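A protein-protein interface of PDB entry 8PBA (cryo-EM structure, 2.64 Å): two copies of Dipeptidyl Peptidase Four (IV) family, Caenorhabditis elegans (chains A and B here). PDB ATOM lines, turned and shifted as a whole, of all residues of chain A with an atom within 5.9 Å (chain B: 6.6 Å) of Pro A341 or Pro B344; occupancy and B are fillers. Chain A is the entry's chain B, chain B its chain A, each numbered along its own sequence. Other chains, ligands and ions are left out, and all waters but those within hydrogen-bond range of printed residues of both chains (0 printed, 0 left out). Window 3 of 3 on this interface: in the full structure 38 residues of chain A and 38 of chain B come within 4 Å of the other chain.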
ATOM      1  N   GLN A 333       0.505  26.648  18.736  1.00  0.00           N
ATOM      2  CA  GLN A 333      -0.389  25.534  18.482  1.00  0.00           C
ATOM      3  C   GLN A 333      -0.460  24.616  19.686  1.00  0.00           C
ATOM      4  O   GLN A 333       0.557  24.323  20.307  1.00  0.00           O
ATOM      5  CB  GLN A 333       0.088  24.738  17.270  1.00  0.00           C
ATOM      6  CG  GLN A 333      -0.838  23.602  16.859  1.00  0.00           C
ATOM      7  CD  GLN A 333      -2.119  24.103  16.233  1.00  0.00           C
ATOM      8  OE1 GLN A 333      -2.082  24.750  15.186  1.00  0.00           O
ATOM      9  NE2 GLN A 333      -3.253  23.848  16.884  1.00  0.00           N
ATOM     10  N   ASP A 339      -3.907  14.468  15.347  1.00  0.00           N
ATOM     11  CA  ASP A 339      -5.297  14.872  15.496  1.00  0.00           C
ATOM     12  C   ASP A 339      -5.556  16.135  14.692  1.00  0.00           C
ATOM     13  O   ASP A 339      -4.604  16.818  14.320  1.00  0.00           O
ATOM     14  CB  ASP A 339      -5.639  15.085  16.966  1.00  0.00           C
ATOM     15  CG  ASP A 339      -5.805  13.787  17.731  1.00  0.00           C
ATOM     16  OD1 ASP A 339      -6.099  12.780  17.129  1.00  0.00           O
ATOM     17  OD2 ASP A 339      -5.701  13.821  18.927  1.00  0.00           O
ATOM     18  N   PRO A 340      -6.818  16.452  14.381  1.00  0.00           N
ATOM     19  CA  PRO A 340      -7.229  17.643  13.671  1.00  0.00           C
ATOM     20  C   PRO A 340      -6.723  18.887  14.394  1.00  0.00           C
ATOM     21  O   PRO A 340      -6.654  18.890  15.622  1.00  0.00           O
ATOM     22  CB  PRO A 340      -8.754  17.550  13.742  1.00  0.00           C
ATOM     23  CG  PRO A 340      -9.039  16.074  13.841  1.00  0.00           C
ATOM     24  CD  PRO A 340      -7.909  15.507  14.660  1.00  0.00           C
ATOM     25  N   PRO A 341      -6.356  19.937  13.654  1.00  0.00           N
ATOM     26  CA  PRO A 341      -5.955  21.238  14.143  1.00  0.00           C
ATOM     27  C   PRO A 341      -7.087  21.922  14.882  1.00  0.00           C
ATOM     28  O   PRO A 341      -8.254  21.784  14.518  1.00  0.00           O
ATOM     29  CB  PRO A 341      -5.623  21.992  12.852  1.00  0.00           C
ATOM     30  CG  PRO A 341      -5.291  20.926  11.852  1.00  0.00           C
ATOM     31  CD  PRO A 341      -6.127  19.742  12.230  1.00  0.00           C
ATOM     32  N   VAL A 342      -6.723  22.723  15.868  1.00  0.00           N
ATOM     33  CA  VAL A 342      -7.665  23.559  16.595  1.00  0.00           C
ATOM     34  C   VAL A 342      -7.164  24.986  16.561  1.00  0.00           C
ATOM     35  O   VAL A 342      -5.990  25.225  16.273  1.00  0.00           O
ATOM     36  CB  VAL A 342      -7.826  23.084  18.049  1.00  0.00           C
ATOM     37  CG1 VAL A 342      -8.351  21.665  18.074  1.00  0.00           C
ATOM     38  CG2 VAL A 342      -6.494  23.178  18.775  1.00  0.00           C
ATOM     39  N   ALA A 343      -8.033  25.936  16.873  1.00  0.00           N
ATOM     40  CA  ALA A 343      -7.641  27.333  16.802  1.00  0.00           C
ATOM     41  C   ALA A 343      -6.356  27.564  17.598  1.00  0.00           C
ATOM     42  O   ALA A 343      -6.264  27.135  18.748  1.00  0.00           O
ATOM     43  CB  ALA A 343      -8.746  28.212  17.358  1.00  0.00           C
ATOM     44  N   LYS B 289      -3.701  23.343  -2.919  1.00  0.00           N
ATOM     45  CA  LYS B 289      -2.645  22.387  -2.622  1.00  0.00           C
ATOM     46  C   LYS B 289      -3.204  20.991  -2.407  1.00  0.00           C
ATOM     47  O   LYS B 289      -2.467  20.006  -2.406  1.00  0.00           O
ATOM     48  CB  LYS B 289      -1.861  22.846  -1.406  1.00  0.00           C
ATOM     49  CG  LYS B 289      -2.636  22.801  -0.119  1.00  0.00           C
ATOM     50  CD  LYS B 289      -1.872  23.480   0.988  1.00  0.00           C
ATOM     51  CE  LYS B 289      -2.681  23.543   2.259  1.00  0.00           C
ATOM     52  NZ  LYS B 289      -2.016  24.364   3.289  1.00  0.00           N
ATOM     53  N   HIS B 290      -4.513  20.915  -2.205  1.00  0.00           N
ATOM     54  CA  HIS B 290      -5.187  19.656  -1.940  1.00  0.00           C
ATOM     55  C   HIS B 290      -5.707  19.020  -3.217  1.00  0.00           C
ATOM     56  O   HIS B 290      -6.378  17.987  -3.183  1.00  0.00           O
ATOM     57  CB  HIS B 290      -6.334  19.880  -0.967  1.00  0.00           C
ATOM     58  CG  HIS B 290      -5.869  20.319   0.359  1.00  0.00           C
ATOM     59  ND1 HIS B 290      -6.566  21.218   1.127  1.00  0.00           N
ATOM     60  CD2 HIS B 290      -4.765  19.996   1.063  1.00  0.00           C
ATOM     61  CE1 HIS B 290      -5.909  21.431   2.246  1.00  0.00           C
ATOM     62  NE2 HIS B 290      -4.816  20.698   2.232  1.00  0.00           N
ATOM     63  N   GLU B 331      -7.747  16.119   8.559  1.00  0.00           N
ATOM     64  CA  GLU B 331      -6.471  16.744   8.868  1.00  0.00           C
ATOM     65  C   GLU B 331      -5.742  16.090  10.027  1.00  0.00           C
ATOM     66  O   GLU B 331      -6.363  15.605  10.973  1.00  0.00           O
ATOM     67  CB  GLU B 331      -6.699  18.200   9.213  1.00  0.00           C
ATOM     68  CG  GLU B 331      -7.348  18.980   8.126  1.00  0.00           C
ATOM     69  CD  GLU B 331      -8.824  18.719   8.051  1.00  0.00           C
ATOM     70  OE1 GLU B 331      -9.398  18.984   7.023  1.00  0.00           O
ATOM     71  OE2 GLU B 331      -9.364  18.189   8.995  1.00  0.00           O
ATOM     72  N   SER B 332      -4.421  16.183   9.988  1.00  0.00           N
ATOM     73  CA  SER B 332      -3.560  15.815  11.096  1.00  0.00           C
ATOM     74  C   SER B 332      -2.515  16.891  11.341  1.00  0.00           C
ATOM     75  O   SER B 332      -1.720  17.219  10.459  1.00  0.00           O
ATOM     76  CB  SER B 332      -2.876  14.498  10.813  1.00  0.00           C
ATOM     77  OG  SER B 332      -3.785  13.434  10.859  1.00  0.00           O
ATOM     78  N   GLN B 333      -2.493  17.429  12.545  1.00  0.00           N
ATOM     79  CA  GLN B 333      -1.537  18.467  12.882  1.00  0.00           C
ATOM     80  C   GLN B 333      -0.227  17.862  13.344  1.00  0.00           C
ATOM     81  O   GLN B 333      -0.221  16.897  14.102  1.00  0.00           O
ATOM     82  CB  GLN B 333      -2.095  19.363  13.984  1.00  0.00           C
ATOM     83  CG  GLN B 333      -1.208  20.546  14.344  1.00  0.00           C
ATOM     84  CD  GLN B 333      -1.195  21.603  13.263  1.00  0.00           C
ATOM     85  OE1 GLN B 333      -2.234  22.190  12.960  1.00  0.00           O
ATOM     86  NE2 GLN B 333      -0.034  21.826  12.647  1.00  0.00           N
ATOM     87  N   PHE B 334       0.879  18.415  12.875  1.00  0.00           N
ATOM     88  CA  PHE B 334       2.185  18.041  13.393  1.00  0.00           C
ATOM     89  C   PHE B 334       2.946  19.265  13.848  1.00  0.00           C
ATOM     90  O   PHE B 334       2.693  20.373  13.377  1.00  0.00           O
ATOM     91  CB  PHE B 334       2.994  17.270  12.365  1.00  0.00           C
ATOM     92  CG  PHE B 334       2.420  15.951  12.085  1.00  0.00           C
ATOM     93  CD1 PHE B 334       1.543  15.772  11.059  1.00  0.00           C
ATOM     94  CD2 PHE B 334       2.715  14.895  12.889  1.00  0.00           C
ATOM     95  CE1 PHE B 334       0.969  14.560  10.850  1.00  0.00           C
ATOM     96  CE2 PHE B 334       2.142  13.688  12.682  1.00  0.00           C
ATOM     97  CZ  PHE B 334       1.262  13.526  11.664  1.00  0.00           C
ATOM     98  N   VAL B 342       1.837  24.916  11.511  1.00  0.00           N
ATOM     99  CA  VAL B 342       2.322  24.643  10.168  1.00  0.00           C
ATOM    100  C   VAL B 342       1.219  23.955   9.392  1.00  0.00           C
ATOM    101  O   VAL B 342       0.274  23.436   9.988  1.00  0.00           O
ATOM    102  CB  VAL B 342       3.583  23.764  10.195  1.00  0.00           C
ATOM    103  CG1 VAL B 342       4.689  24.471  10.950  1.00  0.00           C
ATOM    104  CG2 VAL B 342       3.266  22.422  10.836  1.00  0.00           C
ATOM    105  N   ALA B 343       1.340  23.925   8.073  1.00  0.00           N
ATOM    106  CA  ALA B 343       0.291  23.336   7.260  1.00  0.00           C
ATOM    107  C   ALA B 343      -0.036  21.926   7.755  1.00  0.00           C
ATOM    108  O   ALA B 343       0.875  21.122   7.956  1.00  0.00           O
ATOM    109  CB  ALA B 343       0.730  23.274   5.809  1.00  0.00           C
ATOM    110  N   PRO B 344      -1.323  21.611   7.952  1.00  0.00           N
ATOM    111  CA  PRO B 344      -1.837  20.313   8.332  1.00  0.00           C
ATOM    112  C   PRO B 344      -1.566  19.271   7.270  1.00  0.00           C
ATOM    113  O   PRO B 344      -1.594  19.558   6.074  1.00  0.00           O
ATOM    114  CB  PRO B 344      -3.337  20.568   8.477  1.00  0.00           C
ATOM    115  CG  PRO B 344      -3.449  22.033   8.776  1.00  0.00           C
ATOM    116  CD  PRO B 344      -2.308  22.687   8.046  1.00  0.00           C
ATOM    117  N   MET B 345      -1.368  18.048   7.722  1.00  0.00           N
ATOM    118  CA  MET B 345      -1.216  16.894   6.860  1.00  0.00           C
ATOM    119  C   MET B 345      -2.591  16.338   6.540  1.00  0.00           C
ATOM    120  O   MET B 345      -3.460  16.295   7.406  1.00  0.00           O
ATOM    121  CB  MET B 345      -0.378  15.862   7.612  1.00  0.00           C
ATOM    122  CG  MET B 345      -0.102  14.552   6.920  1.00  0.00           C
ATOM    123  SD  MET B 345       0.990  14.700   5.529  1.00  0.00           S
ATOM    124  CE  MET B 345       0.912  13.014   4.932  1.00  0.00           C
ATOM    125  N   LYS B 346      -2.795  15.886   5.317  1.00  0.00           N
ATOM    126  CA  LYS B 346      -4.031  15.184   5.008  1.00  0.00           C
ATOM    127  C   LYS B 346      -3.845  13.692   5.191  1.00  0.00           C
ATOM    128  O   LYS B 346      -3.023  13.070   4.519  1.00  0.00           O
ATOM    129  CB  LYS B 346      -4.512  15.521   3.606  1.00  0.00           C
ATOM    130  CG  LYS B 346      -5.056  16.937   3.438  1.00  0.00           C
ATOM    131  CD  LYS B 346      -6.373  17.105   4.205  1.00  0.00           C
ATOM    132  CE  LYS B 346      -7.180  18.272   3.685  1.00  0.00           C
ATOM    133  NZ  LYS B 346      -8.528  18.351   4.305  1.00  0.00           N
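The side-chain amide oxygen (OE1) of Gln B333 sits close to the side-chain amide oxygen (OE1) of Gln A333 (3.4 Å). The backbone NH (N) of Gln B333 lies within hydrogen-bond range of the backbone carbonyl oxygen (O) of Asp A339 (2.8 Å).
The side-chain carboxylate of Glu B331 lies within salt-bridge range of the side-chain amino group of Lys B346 (2.9 Å). The backbone NH (N) of Ser B332 sits at hydrogen-bond distance from the backbone carbonyl oxygen (O) of Met B345 (2.8 Å). The side-chain amide nitrogen (NE2) of Gln B333 is in hydrogen-bond range of the backbone carbonyl oxygen (O) of Val B342 (3.1 Å). The side-chain amide nitrogen (NE2) of Gln A333 lies within hydrogen-bond range of the backbone carbonyl oxygen (O) of Val A342 (3.1 Å).
O of Glu B331 touches C of Asp A339, 3.8 Å away. Asp A339 touches Ser B332. CA of Pro A340 touches O of Glu B331, at 3.5 Å. Glu B331 touches Pro A341. CB of Pro A341 touches OE1 of Gln B333, 3.4 Å away. Pro A341 touches Pro B344.
Of the printed residues of chain B, Asp A339 touches Glu B331, Ser B332 and Gln B333. Printed residues of chain B within 4 Å of Pro A340: Glu B331 (3.5 Å). Of the printed residues of chain A, Glu B331 touches Asp A339 (3.8 Å), Pro A340 (3.5 Å) and Pro A341 (3.4 Å). Of the printed residues of chain A, Ser B332 touches Asp A339. Printed residues of chain A within 4 Å of Gln B333: Gln A333 (3.4 Å), Asp A339 (2.8 Å) and Pro A341 (3.4 Å). Val B342 touches none of the printed residues of chain A. Of chain A, only Pro A341 (3.8 Å) comes within 4 Å of Pro B344. The nearest printed residue of chain A that does not touch Pro B344 is Pro A340 (7.0 Å).
Of the 11 printed residues of chain B, 4 touch a printed residue of chain A. Hydrophobic or aromatic side chains of chain B that line the printed part of chain A: Pro B344. Of the 6 printed residues of chain A, 4 touch a printed residue of chain B. Hydrophobic or aromatic side chains of chain A that line the printed part of chain B: Pro A340 and Pro A341. Among the printed residues, no Asp or Glu carboxylate lies within 4 Å of a Lys or Arg side-chain nitrogen of the other chain.
Gln A333 touches its own counterpart, Gln B333. Positions printed for both chains: 333, 342 and 343.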
